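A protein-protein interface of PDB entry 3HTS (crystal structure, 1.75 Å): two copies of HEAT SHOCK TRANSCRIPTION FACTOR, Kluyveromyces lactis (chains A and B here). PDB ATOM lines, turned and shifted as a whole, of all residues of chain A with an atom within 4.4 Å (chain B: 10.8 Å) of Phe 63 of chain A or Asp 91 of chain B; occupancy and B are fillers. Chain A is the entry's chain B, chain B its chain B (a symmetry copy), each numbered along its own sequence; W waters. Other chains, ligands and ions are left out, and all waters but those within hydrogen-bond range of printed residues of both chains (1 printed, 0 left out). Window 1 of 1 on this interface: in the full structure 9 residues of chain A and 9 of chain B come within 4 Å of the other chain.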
ATOM      1  N   ARG A  46       4.271 -11.199 -12.722  1.00  0.00           N
ATOM      2  CA  ARG A  46       5.318 -11.290 -11.730  1.00  0.00           C
ATOM      3  C   ARG A  46       6.062 -12.631 -11.739  1.00  0.00           C
ATOM      4  O   ARG A  46       7.283 -12.679 -11.670  1.00  0.00           O
ATOM      5  CB  ARG A  46       4.698 -11.032 -10.365  1.00  0.00           C
ATOM      6  CG  ARG A  46       5.595 -11.378  -9.205  1.00  0.00           C
ATOM      7  CD  ARG A  46       5.016 -10.824  -7.932  1.00  0.00           C
ATOM      8  NE  ARG A  46       3.618 -11.190  -7.798  1.00  0.00           N
ATOM      9  CZ  ARG A  46       3.215 -12.372  -7.365  1.00  0.00           C
ATOM     10  NH1 ARG A  46       4.113 -13.286  -7.026  1.00  0.00           N
ATOM     11  NH2 ARG A  46       1.919 -12.643  -7.295  1.00  0.00           N
ATOM     12  N   PHE A  49       8.345 -12.994 -14.785  1.00  0.00           N
ATOM     13  CA  PHE A  49       9.420 -12.019 -14.561  1.00  0.00           C
ATOM     14  C   PHE A  49      10.458 -12.536 -13.524  1.00  0.00           C
ATOM     15  O   PHE A  49      11.670 -12.441 -13.746  1.00  0.00           O
ATOM     16  CB  PHE A  49       8.807 -10.680 -14.124  1.00  0.00           C
ATOM     17  CG  PHE A  49       9.818  -9.669 -13.671  1.00  0.00           C
ATOM     18  CD1 PHE A  49      10.562  -8.949 -14.601  1.00  0.00           C
ATOM     19  CD2 PHE A  49      10.035  -9.441 -12.305  1.00  0.00           C
ATOM     20  CE1 PHE A  49      11.516  -8.012 -14.180  1.00  0.00           C
ATOM     21  CE2 PHE A  49      10.981  -8.513 -11.873  1.00  0.00           C
ATOM     22  CZ  PHE A  49      11.722  -7.798 -12.817  1.00  0.00           C
ATOM     23  N   VAL A  50       9.999 -13.068 -12.392  1.00  0.00           N
ATOM     24  CA  VAL A  50      10.915 -13.606 -11.407  1.00  0.00           C
ATOM     25  C   VAL A  50      11.692 -14.805 -11.975  1.00  0.00           C
ATOM     26  O   VAL A  50      12.877 -14.973 -11.714  1.00  0.00           O
ATOM     27  CB  VAL A  50      10.174 -14.045 -10.130  1.00  0.00           C
ATOM     28  CG1 VAL A  50      11.075 -14.907  -9.290  1.00  0.00           C
ATOM     29  CG2 VAL A  50       9.797 -12.834  -9.306  1.00  0.00           C
ATOM     30  N   LEU A  54      14.788 -11.767 -13.315  1.00  0.00           N
ATOM     31  CA  LEU A  54      15.616 -11.543 -12.125  1.00  0.00           C
ATOM     32  C   LEU A  54      16.935 -12.319 -12.069  1.00  0.00           C
ATOM     33  O   LEU A  54      17.972 -11.753 -11.746  1.00  0.00           O
ATOM     34  CB  LEU A  54      14.788 -11.765 -10.850  1.00  0.00           C
ATOM     35  CG  LEU A  54      13.771 -10.644 -10.569  1.00  0.00           C
ATOM     36  CD1 LEU A  54      13.032 -10.927  -9.262  1.00  0.00           C
ATOM     37  CD2 LEU A  54      14.482  -9.285 -10.513  1.00  0.00           C
ATOM     38  N   SER A  61      16.709 -14.463  -6.773  1.00  0.00           N
ATOM     39  CA  SER A  61      15.502 -13.954  -7.426  1.00  0.00           C
ATOM     40  C   SER A  61      14.427 -13.818  -6.343  1.00  0.00           C
ATOM     41  O   SER A  61      13.817 -14.798  -5.956  1.00  0.00           O
ATOM     42  CB  SER A  61      15.025 -14.932  -8.490  1.00  0.00           C
ATOM     43  OG  SER A  61      15.628 -14.621  -9.731  1.00  0.00           O
ATOM     44  N   ASN A  62      14.201 -12.600  -5.874  1.00  0.00           N
ATOM     45  CA  ASN A  62      13.238 -12.336  -4.797  1.00  0.00           C
ATOM     46  C   ASN A  62      12.463 -11.063  -5.206  1.00  0.00           C
ATOM     47  O   ASN A  62      12.983  -9.950  -5.153  1.00  0.00           O
ATOM     48  CB  ASN A  62      14.039 -12.130  -3.504  1.00  0.00           C
ATOM     49  CG  ASN A  62      13.172 -11.988  -2.262  1.00  0.00           C
ATOM     50  OD1 ASN A  62      13.426 -12.636  -1.235  1.00  0.00           O
ATOM     51  ND2 ASN A  62      12.174 -11.126  -2.331  1.00  0.00           N
ATOM     52  N   PHE A  63      11.224 -11.228  -5.648  1.00  0.00           N
ATOM     53  CA  PHE A  63      10.413 -10.083  -6.091  1.00  0.00           C
ATOM     54  C   PHE A  63      10.229  -9.031  -4.991  1.00  0.00           C
ATOM     55  O   PHE A  63      10.257  -7.811  -5.257  1.00  0.00           O
ATOM     56  CB  PHE A  63       9.033 -10.563  -6.567  1.00  0.00           C
ATOM     57  CG  PHE A  63       8.316  -9.565  -7.421  1.00  0.00           C
ATOM     58  CD1 PHE A  63       8.751  -9.298  -8.718  1.00  0.00           C
ATOM     59  CD2 PHE A  63       7.218  -8.864  -6.915  1.00  0.00           C
ATOM     60  CE1 PHE A  63       8.105  -8.329  -9.517  1.00  0.00           C
ATOM     61  CE2 PHE A  63       6.561  -7.895  -7.701  1.00  0.00           C
ATOM     62  CZ  PHE A  63       7.019  -7.631  -9.015  1.00  0.00           C
ATOM     63  N   ALA A  64      10.056  -9.489  -3.754  1.00  0.00           N
ATOM     64  CA  ALA A  64       9.851  -8.567  -2.638  1.00  0.00           C
ATOM     65  C   ALA A  64      11.082  -7.652  -2.455  1.00  0.00           C
ATOM     66  O   ALA A  64      10.959  -6.461  -2.141  1.00  0.00           O
ATOM     67  CB  ALA A  64       9.584  -9.364  -1.354  1.00  0.00           C
ATOM     68  N   SER A  65      12.271  -8.225  -2.647  1.00  0.00           N
ATOM     69  CA  SER A  65      13.482  -7.444  -2.506  1.00  0.00           C
ATOM     70  C   SER A  65      13.555  -6.464  -3.646  1.00  0.00           C
ATOM     71  O   SER A  65      14.073  -5.362  -3.468  1.00  0.00           O
ATOM     72  CB  SER A  65      14.700  -8.344  -2.488  1.00  0.00           C
ATOM     73  OG  SER A  65      14.720  -8.982  -1.233  1.00  0.00           O
ATOM     74  N   PHE A  66      13.028  -6.864  -4.810  1.00  0.00           N
ATOM     75  CA  PHE A  66      13.014  -5.988  -6.001  1.00  0.00           C
ATOM     76  C   PHE A  66      12.089  -4.790  -5.729  1.00  0.00           C
ATOM     77  O   PHE A  66      12.489  -3.632  -5.838  1.00  0.00           O
ATOM     78  CB  PHE A  66      12.563  -6.818  -7.223  1.00  0.00           C
ATOM     79  CG  PHE A  66      12.545  -6.057  -8.542  1.00  0.00           C
ATOM     80  CD1 PHE A  66      13.740  -5.659  -9.169  1.00  0.00           C
ATOM     81  CD2 PHE A  66      11.337  -5.791  -9.171  1.00  0.00           C
ATOM     82  CE1 PHE A  66      13.708  -5.007 -10.404  1.00  0.00           C
ATOM     83  CE2 PHE A  66      11.288  -5.148 -10.399  1.00  0.00           C
ATOM     84  CZ  PHE A  66      12.466  -4.752 -11.023  1.00  0.00           C
ATOM     85  N   VAL A  67      10.859  -5.065  -5.322  1.00  0.00           N
ATOM     86  CA  VAL A  67       9.901  -4.014  -5.014  1.00  0.00           C
ATOM     87  C   VAL A  67      10.460  -3.115  -3.899  1.00  0.00           C
ATOM     88  O   VAL A  67      10.364  -1.897  -3.977  1.00  0.00           O
ATOM     89  CB  VAL A  67       8.566  -4.632  -4.550  1.00  0.00           C
ATOM     90  CG1 VAL A  67       7.605  -3.542  -4.135  1.00  0.00           C
ATOM     91  CG2 VAL A  67       7.967  -5.460  -5.673  1.00  0.00           C
ATOM     92  N   TRP A  94       2.053  -6.003 -12.111  1.00  0.00           N
ATOM     93  CA  TRP A  94       2.636  -4.905 -11.368  1.00  0.00           C
ATOM     94  C   TRP A  94       3.064  -3.813 -12.301  1.00  0.00           C
ATOM     95  O   TRP A  94       3.630  -4.080 -13.337  1.00  0.00           O
ATOM     96  CB  TRP A  94       3.873  -5.382 -10.629  1.00  0.00           C
ATOM     97  CG  TRP A  94       3.557  -6.349  -9.564  1.00  0.00           C
ATOM     98  CD1 TRP A  94       3.147  -7.642  -9.724  1.00  0.00           C
ATOM     99  CD2 TRP A  94       3.619  -6.113  -8.153  1.00  0.00           C
ATOM    100  NE1 TRP A  94       2.948  -8.219  -8.496  1.00  0.00           N
ATOM    101  CE2 TRP A  94       3.232  -7.301  -7.514  1.00  0.00           C
ATOM    102  CE3 TRP A  94       3.970  -5.005  -7.367  1.00  0.00           C
ATOM    103  CZ2 TRP A  94       3.184  -7.424  -6.126  1.00  0.00           C
ATOM    104  CZ3 TRP A  94       3.923  -5.131  -5.981  1.00  0.00           C
ATOM    105  CH2 TRP A  94       3.531  -6.328  -5.379  1.00  0.00           C
ATOM    106  N   VAL B  43       5.261 -23.687   3.826  1.00  0.00           N
ATOM    107  CA  VAL B  43       4.618 -23.441   2.549  1.00  0.00           C
ATOM    108  C   VAL B  43       5.733 -23.844   1.590  1.00  0.00           C
ATOM    109  O   VAL B  43       6.613 -23.049   1.259  1.00  0.00           O
ATOM    110  CB  VAL B  43       4.265 -21.955   2.326  1.00  0.00           C
ATOM    111  CG1 VAL B  43       3.965 -21.725   0.842  1.00  0.00           C
ATOM    112  CG2 VAL B  43       3.050 -21.565   3.178  1.00  0.00           C
ATOM    113  N   PRO B  44       5.725 -25.117   1.168  1.00  0.00           N
ATOM    114  CA  PRO B  44       6.739 -25.645   0.254  1.00  0.00           C
ATOM    115  C   PRO B  44       6.910 -24.798  -0.990  1.00  0.00           C
ATOM    116  O   PRO B  44       8.034 -24.500  -1.377  1.00  0.00           O
ATOM    117  CB  PRO B  44       6.232 -27.055  -0.066  1.00  0.00           C
ATOM    118  CG  PRO B  44       5.371 -27.421   1.119  1.00  0.00           C
ATOM    119  CD  PRO B  44       4.725 -26.141   1.537  1.00  0.00           C
ATOM    120  N   ASN B  45       5.796 -24.406  -1.601  1.00  0.00           N
ATOM    121  CA  ASN B  45       5.822 -23.622  -2.823  1.00  0.00           C
ATOM    122  C   ASN B  45       4.827 -22.491  -2.778  1.00  0.00           C
ATOM    123  O   ASN B  45       3.622 -22.696  -2.904  1.00  0.00           O
ATOM    124  CB  ASN B  45       5.503 -24.503  -4.028  1.00  0.00           C
ATOM    125  CG  ASN B  45       5.718 -23.788  -5.340  1.00  0.00           C
ATOM    126  OD1 ASN B  45       4.824 -23.114  -5.843  1.00  0.00           O
ATOM    127  ND2 ASN B  45       6.910 -23.924  -5.897  1.00  0.00           N
ATOM    128  N   ARG B  46       5.348 -21.287  -2.607  1.00  0.00           N
ATOM    129  CA  ARG B  46       4.526 -20.100  -2.530  1.00  0.00           C
ATOM    130  C   ARG B  46       3.535 -19.959  -3.692  1.00  0.00           C
ATOM    131  O   ARG B  46       2.370 -19.639  -3.495  1.00  0.00           O
ATOM    132  CB  ARG B  46       5.448 -18.892  -2.466  1.00  0.00           C
ATOM    133  CG  ARG B  46       4.752 -17.573  -2.676  1.00  0.00           C
ATOM    134  CD  ARG B  46       5.677 -16.445  -2.308  1.00  0.00           C
ATOM    135  NE  ARG B  46       6.967 -16.604  -2.955  1.00  0.00           N
ATOM    136  CZ  ARG B  46       7.196 -16.267  -4.213  1.00  0.00           C
ATOM    137  NH1 ARG B  46       6.216 -15.753  -4.941  1.00  0.00           N
ATOM    138  NH2 ARG B  46       8.395 -16.468  -4.743  1.00  0.00           N
ATOM    139  N   GLU B  47       4.001 -20.214  -4.906  1.00  0.00           N
ATOM    140  CA  GLU B  47       3.172 -20.097  -6.110  1.00  0.00           C
ATOM    141  C   GLU B  47       1.919 -20.990  -6.098  1.00  0.00           C
ATOM    142  O   GLU B  47       0.826 -20.543  -6.438  1.00  0.00           O
ATOM    143  CB  GLU B  47       4.008 -20.456  -7.346  1.00  0.00           C
ATOM    144  CG  GLU B  47       4.699 -19.303  -7.979  1.00  0.00           C
ATOM    145  CD  GLU B  47       5.833 -18.784  -7.130  1.00  0.00           C
ATOM    146  OE1 GLU B  47       6.559 -19.591  -6.480  1.00  0.00           O
ATOM    147  OE2 GLU B  47       5.992 -17.548  -7.117  1.00  0.00           O
ATOM    148  N   ARG B  48       2.117 -22.259  -5.755  1.00  0.00           N
ATOM    149  CA  ARG B  48       1.039 -23.250  -5.691  1.00  0.00           C
ATOM    150  C   ARG B  48       0.092 -22.849  -4.592  1.00  0.00           C
ATOM    151  O   ARG B  48      -1.116 -22.909  -4.765  1.00  0.00           O
ATOM    152  CB  ARG B  48       1.584 -24.634  -5.355  1.00  0.00           C
ATOM    153  CG  ARG B  48       2.451 -25.260  -6.409  1.00  0.00           C
ATOM    154  CD  ARG B  48       2.752 -26.702  -6.020  1.00  0.00           C
ATOM    155  NE  ARG B  48       4.009 -27.159  -6.597  1.00  0.00           N
ATOM    156  CZ  ARG B  48       5.023 -27.659  -5.894  1.00  0.00           C
ATOM    157  NH1 ARG B  48       4.942 -27.779  -4.570  1.00  0.00           N
ATOM    158  NH2 ARG B  48       6.133 -28.030  -6.523  1.00  0.00           N
ATOM    159  N   PHE B  49       0.660 -22.468  -3.448  1.00  0.00           N
ATOM    160  CA  PHE B  49      -0.123 -22.024  -2.287  1.00  0.00           C
ATOM    161  C   PHE B  49      -1.014 -20.796  -2.631  1.00  0.00           C
ATOM    162  O   PHE B  49      -2.199 -20.763  -2.284  1.00  0.00           O
ATOM    163  CB  PHE B  49       0.830 -21.719  -1.121  1.00  0.00           C
ATOM    164  CG  PHE B  49       0.162 -21.064   0.052  1.00  0.00           C
ATOM    165  CD1 PHE B  49      -0.589 -21.818   0.948  1.00  0.00           C
ATOM    166  CD2 PHE B  49       0.277 -19.682   0.256  1.00  0.00           C
ATOM    167  CE1 PHE B  49      -1.224 -21.205   2.038  1.00  0.00           C
ATOM    168  CE2 PHE B  49      -0.350 -19.061   1.335  1.00  0.00           C
ATOM    169  CZ  PHE B  49      -1.102 -19.829   2.227  1.00  0.00           C
ATOM    170  N   VAL B  50      -0.457 -19.786  -3.296  1.00  0.00           N
ATOM    171  CA  VAL B  50      -1.246 -18.634  -3.683  1.00  0.00           C
ATOM    172  C   VAL B  50      -2.353 -19.033  -4.673  1.00  0.00           C
ATOM    173  O   VAL B  50      -3.469 -18.533  -4.610  1.00  0.00           O
ATOM    174  CB  VAL B  50      -0.370 -17.539  -4.320  1.00  0.00           C
ATOM    175  CG1 VAL B  50      -1.241 -16.533  -5.019  1.00  0.00           C
ATOM    176  CG2 VAL B  50       0.408 -16.807  -3.248  1.00  0.00           C
ATOM    177  N   ASN B  62      -3.069 -12.538  -2.289  1.00  0.00           N
ATOM    178  CA  ASN B  62      -1.875 -11.683  -2.274  1.00  0.00           C
ATOM    179  C   ASN B  62      -0.952 -12.239  -1.166  1.00  0.00           C
ATOM    180  O   ASN B  62      -1.209 -12.076   0.025  1.00  0.00           O
ATOM    181  CB  ASN B  62      -2.337 -10.251  -1.969  1.00  0.00           C
ATOM    182  CG  ASN B  62      -1.228  -9.215  -2.063  1.00  0.00           C
ATOM    183  OD1 ASN B  62      -1.398  -8.159  -2.692  1.00  0.00           O
ATOM    184  ND2 ASN B  62      -0.109  -9.486  -1.417  1.00  0.00           N
ATOM    185  N   PHE B  63       0.111 -12.928  -1.557  1.00  0.00           N
ATOM    186  CA  PHE B  63       1.035 -13.525  -0.580  1.00  0.00           C
ATOM    187  C   PHE B  63       1.651 -12.484   0.362  1.00  0.00           C
ATOM    188  O   PHE B  63       1.822 -12.735   1.574  1.00  0.00           O
ATOM    189  CB  PHE B  63       2.161 -14.278  -1.306  1.00  0.00           C
ATOM    190  CG  PHE B  63       2.882 -15.259  -0.435  1.00  0.00           C
ATOM    191  CD1 PHE B  63       2.259 -16.437  -0.027  1.00  0.00           C
ATOM    192  CD2 PHE B  63       4.180 -14.988   0.006  1.00  0.00           C
ATOM    193  CE1 PHE B  63       2.917 -17.349   0.828  1.00  0.00           C
ATOM    194  CE2 PHE B  63       4.850 -15.891   0.858  1.00  0.00           C
ATOM    195  CZ  PHE B  63       4.201 -17.081   1.268  1.00  0.00           C
ATOM    196  N   ALA B  64       1.971 -11.311  -0.177  1.00  0.00           N
ATOM    197  CA  ALA B  64       2.583 -10.259   0.633  1.00  0.00           C
ATOM    198  C   ALA B  64       1.630  -9.822   1.768  1.00  0.00           C
ATOM    199  O   ALA B  64       2.058  -9.537   2.894  1.00  0.00           O
ATOM    200  CB  ALA B  64       2.932  -9.060  -0.260  1.00  0.00           C
ATOM    201  N   VAL B  67       1.801 -12.666   4.385  1.00  0.00           N
ATOM    202  CA  VAL B  67       2.997 -12.559   5.205  1.00  0.00           C
ATOM    203  C   VAL B  67       2.873 -11.350   6.147  1.00  0.00           C
ATOM    204  O   VAL B  67       3.200 -11.443   7.323  1.00  0.00           O
ATOM    205  CB  VAL B  67       4.241 -12.384   4.311  1.00  0.00           C
ATOM    206  CG1 VAL B  67       5.470 -12.172   5.165  1.00  0.00           C
ATOM    207  CG2 VAL B  67       4.417 -13.609   3.431  1.00  0.00           C
ATOM    208  N   LYS B  77       9.462 -15.473   9.997  1.00  0.00           N
ATOM    209  CA  LYS B  77       9.986 -16.366   8.988  1.00  0.00           C
ATOM    210  C   LYS B  77      11.229 -17.035   9.566  1.00  0.00           C
ATOM    211  O   LYS B  77      12.076 -16.386  10.179  1.00  0.00           O
ATOM    212  CB  LYS B  77      10.369 -15.601   7.743  1.00  0.00           C
ATOM    213  CG  LYS B  77      10.851 -16.496   6.649  1.00  0.00           C
ATOM    214  CD  LYS B  77      10.892 -15.746   5.350  1.00  0.00           C
ATOM    215  CE  LYS B  77      11.599 -16.562   4.316  1.00  0.00           C
ATOM    216  NZ  LYS B  77      11.249 -15.976   3.028  1.00  0.00           N
ATOM    217  N   ASN B  89      19.161 -19.496  -6.089  1.00  0.00           N
ATOM    218  CA  ASN B  89      18.275 -19.452  -4.891  1.00  0.00           C
ATOM    219  C   ASN B  89      17.016 -18.600  -5.132  1.00  0.00           C
ATOM    220  O   ASN B  89      17.104 -17.471  -5.621  1.00  0.00           O
ATOM    221  CB  ASN B  89      19.054 -18.903  -3.699  1.00  0.00           C
ATOM    222  CG  ASN B  89      18.155 -18.529  -2.545  1.00  0.00           C
ATOM    223  OD1 ASN B  89      18.367 -17.518  -1.879  1.00  0.00           O
ATOM    224  ND2 ASN B  89      17.137 -19.347  -2.299  1.00  0.00           N
ATOM    225  N   ASN B  90      15.848 -19.141  -4.779  1.00  0.00           N
ATOM    226  CA  ASN B  90      14.587 -18.424  -4.975  1.00  0.00           C
ATOM    227  C   ASN B  90      13.727 -18.204  -3.723  1.00  0.00           C
ATOM    228  O   ASN B  90      13.998 -18.743  -2.637  1.00  0.00           O
ATOM    229  CB  ASN B  90      13.743 -19.123  -6.058  1.00  0.00           C
ATOM    230  CG  ASN B  90      13.335 -20.551  -5.677  1.00  0.00           C
ATOM    231  OD1 ASN B  90      13.457 -20.971  -4.525  1.00  0.00           O
ATOM    232  ND2 ASN B  90      12.838 -21.297  -6.656  1.00  0.00           N
ATOM    233  N   ASP B  91      12.689 -17.390  -3.906  1.00  0.00           N
ATOM    234  CA  ASP B  91      11.735 -17.052  -2.849  1.00  0.00           C
ATOM    235  C   ASP B  91      10.508 -18.015  -2.873  1.00  0.00           C
ATOM    236  O   ASP B  91       9.412 -17.635  -2.491  1.00  0.00           O
ATOM    237  CB  ASP B  91      11.303 -15.565  -3.019  1.00  0.00           C
ATOM    238  CG  ASP B  91      10.883 -15.220  -4.460  1.00  0.00           C
ATOM    239  OD1 ASP B  91      10.981 -16.088  -5.331  1.00  0.00           O
ATOM    240  OD2 ASP B  91      10.435 -14.088  -4.740  1.00  0.00           O
ATOM    241  N   SER B  92      10.732 -19.263  -3.302  1.00  0.00           N
ATOM    242  CA  SER B  92       9.692 -20.300  -3.430  1.00  0.00           C
ATOM    243  C   SER B  92       9.154 -20.940  -2.156  1.00  0.00           C
ATOM    244  O   SER B  92       7.953 -21.061  -1.994  1.00  0.00           O
ATOM    245  CB  SER B  92      10.199 -21.420  -4.335  1.00  0.00           C
ATOM    246  OG  SER B  92       9.447 -21.470  -5.528  1.00  0.00           O
ATOM    247  N   ARG B  93      10.047 -21.385  -1.283  1.00  0.00           N
ATOM    248  CA  ARG B  93       9.658 -22.003  -0.037  1.00  0.00           C
ATOM    249  C   ARG B  93       9.664 -21.006   1.128  1.00  0.00           C
ATOM    250  O   ARG B  93      10.538 -20.153   1.229  1.00  0.00           O
ATOM    251  CB  ARG B  93      10.591 -23.162   0.283  1.00  0.00           C
ATOM    252  CG  ARG B  93      10.386 -23.713   1.679  1.00  0.00           C
ATOM    253  CD  ARG B  93      11.450 -24.733   2.000  1.00  0.00           C
ATOM    254  NE  ARG B  93      10.938 -25.913   2.692  1.00  0.00           N
ATOM    255  CZ  ARG B  93      10.343 -26.943   2.089  1.00  0.00           C
ATOM    256  NH1 ARG B  93      10.170 -26.954   0.762  1.00  0.00           N
ATOM    257  NH2 ARG B  93       9.932 -27.974   2.823  1.00  0.00           N
ATOM    258  N   TRP B  94       8.668 -21.132   2.002  1.00  0.00           N
ATOM    259  CA  TRP B  94       8.487 -20.280   3.159  1.00  0.00           C
ATOM    260  C   TRP B  94       8.115 -21.102   4.357  1.00  0.00           C
ATOM    261  O   TRP B  94       7.308 -21.999   4.257  1.00  0.00           O
ATOM    262  CB  TRP B  94       7.353 -19.304   2.909  1.00  0.00           C
ATOM    263  CG  TRP B  94       7.670 -18.330   1.849  1.00  0.00           C
ATOM    264  CD1 TRP B  94       7.763 -18.575   0.510  1.00  0.00           C
ATOM    265  CD2 TRP B  94       7.944 -16.935   2.029  1.00  0.00           C
ATOM    266  NE1 TRP B  94       8.082 -17.417  -0.151  1.00  0.00           N
ATOM    267  CE2 TRP B  94       8.199 -16.394   0.759  1.00  0.00           C
ATOM    268  CE3 TRP B  94       7.996 -16.091   3.147  1.00  0.00           C
ATOM    269  CZ2 TRP B  94       8.499 -15.046   0.566  1.00  0.00           C
ATOM    270  CZ3 TRP B  94       8.295 -14.745   2.952  1.00  0.00           C
ATOM    271  CH2 TRP B  94       8.544 -14.240   1.674  1.00  0.00           C
ATOM    272  N   GLU B  95       8.679 -20.759   5.505  1.00  0.00           N
ATOM    273  CA  GLU B  95       8.412 -21.465   6.754  1.00  0.00           C
ATOM    274  C   GLU B  95       8.260 -20.434   7.866  1.00  0.00           C
ATOM    275  O   GLU B  95       9.095 -19.555   8.010  1.00  0.00           O
ATOM    276  CB  GLU B  95       9.580 -22.392   7.052  1.00  0.00           C
ATOM    277  CG  GLU B  95       9.487 -23.133   8.337  1.00  0.00           C
ATOM    278  CD  GLU B  95      10.646 -24.092   8.473  1.00  0.00           C
ATOM    279  OE1 GLU B  95      11.446 -24.209   7.509  1.00  0.00           O
ATOM    280  OE2 GLU B  95      10.751 -24.727   9.543  1.00  0.00           O
ATOM    281  N   PHE B  96       7.213 -20.554   8.664  1.00  0.00           N
ATOM    282  CA  PHE B  96       6.970 -19.587   9.713  1.00  0.00           C
ATOM    283  C   PHE B  96       6.761 -20.241  11.062  1.00  0.00           C
ATOM    284  O   PHE B  96       6.216 -21.344  11.140  1.00  0.00           O
ATOM    285  CB  PHE B  96       5.736 -18.750   9.363  1.00  0.00           C
ATOM    286  CG  PHE B  96       5.806 -18.090   7.999  1.00  0.00           C
ATOM    287  CD1 PHE B  96       6.427 -16.851   7.838  1.00  0.00           C
ATOM    288  CD2 PHE B  96       5.195 -18.675   6.888  1.00  0.00           C
ATOM    289  CE1 PHE B  96       6.439 -16.189   6.601  1.00  0.00           C
ATOM    290  CE2 PHE B  96       5.202 -18.015   5.640  1.00  0.00           C
ATOM    291  CZ  PHE B  96       5.830 -16.764   5.509  1.00  0.00           C
HETATM  292  O   HOH W   1       9.548 -12.373  -2.704  1.00  0.00           O
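The backbone NH of Ser 61 of chain A sits at hydrogen-bond distance from the backbone carbonyl oxygen of Asn 89 of chain B, 3.2 Å away. The backbone NH of Phe 63 of chain A sits at hydrogen-bond distance from the side-chain carboxylate of Asp 91 of chain B (3.1 Å). The backbone NH (N) of Asp 91 of chain B lies close to the backbone carbonyl oxygen (O) of Ser 61 of chain A, at 3.5 Å.
The indole nitrogen (NE1) of Trp 94 of chain B lies within hydrogen-bond range of the backbone carbonyl oxygen (O) of Asp 91 of chain B (2.7 Å). ND2 of Asn 62 of chain A lies close to N of Ala 64 of chain A (3.0 Å). OD1 of Asp 91 of chain B lies within salt-bridge range of NH2 of Arg 46 of chain B (2.7 Å). N of Ser 92 of chain B sits close to OD1 of Asn 90 of chain B (3.4 Å). The backbone NH (N) of Arg 46 of chain B lies within hydrogen-bond range of the backbone carbonyl oxygen (O) of Ser 92 of chain B (2.7 Å). N of Ser 65 of chain A sits close to ND2 of Asn 62 of chain A (2.9 Å).
NH1 of Arg 46 of chain A touches NH1 of Arg 46 of chain B (3.9 Å). Ser 61 of chain A touches Asn 90 of chain B (O to CA, 3.8 Å). Asn 62 of chain A touches Asp 91 of chain B (CA to OD2, 3.3 Å).
Of the printed residues of chain B, Arg 46 of chain A touches Arg 46. Ser 61 of chain A touches just these residues of chain B: Asn 89 (3.2 Å), Asn 90 (3.8 Å) and Asp 91 (3.2 Å). Asn 62 of chain A touches just one residue of chain B: Asp 91 (3.3 Å). Phe 63 of chain A touches just one residue of chain B: Asp 91. No residue of chain B comes within 4 Å of Trp 94 of chain A. Printed residues of chain A within 4 Å of Arg 46 of chain B: Arg 46. Of the printed residues of chain A, Asn 90 of chain B touches Ser 61 (3.8 Å). Of the printed residues of chain A, Asp 91 of chain B touches Ser 61 (3.2 Å), Asn 62 (3.3 Å) and Phe 63 (3.1 Å). The nearest residue of chain A that does not touch Asp 91 of chain B is Val 50 of chain A (4.1 Å). The nearest printed residue of chain A that does not touch Arg 46 of chain B is Val 50 of chain A (5.5 Å).
Among the printed residues, 6 pairs touch across the chains. Among the printed residues, no Asp or Glu carboxylate lies within 4 Å of a Lys or Arg side-chain nitrogen of the other chain.
Arg 46 of chain B touches its own counterpart, Arg 46 of chain A. 8 positions are printed for both chains. Of the 6 pairs that touch across the chains among the printed residues, 1 has its exchanged pair printed and touching as well.
Water W1 lies within hydrogen-bond range of the side-chain carboxylate of Asp 91 of chain B (2.8 Å), the side-chain amide nitrogen of Asn 62 of chain A (2.9 Å) and the backbone NH of Ala 64 of chain A (3.1 Å).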
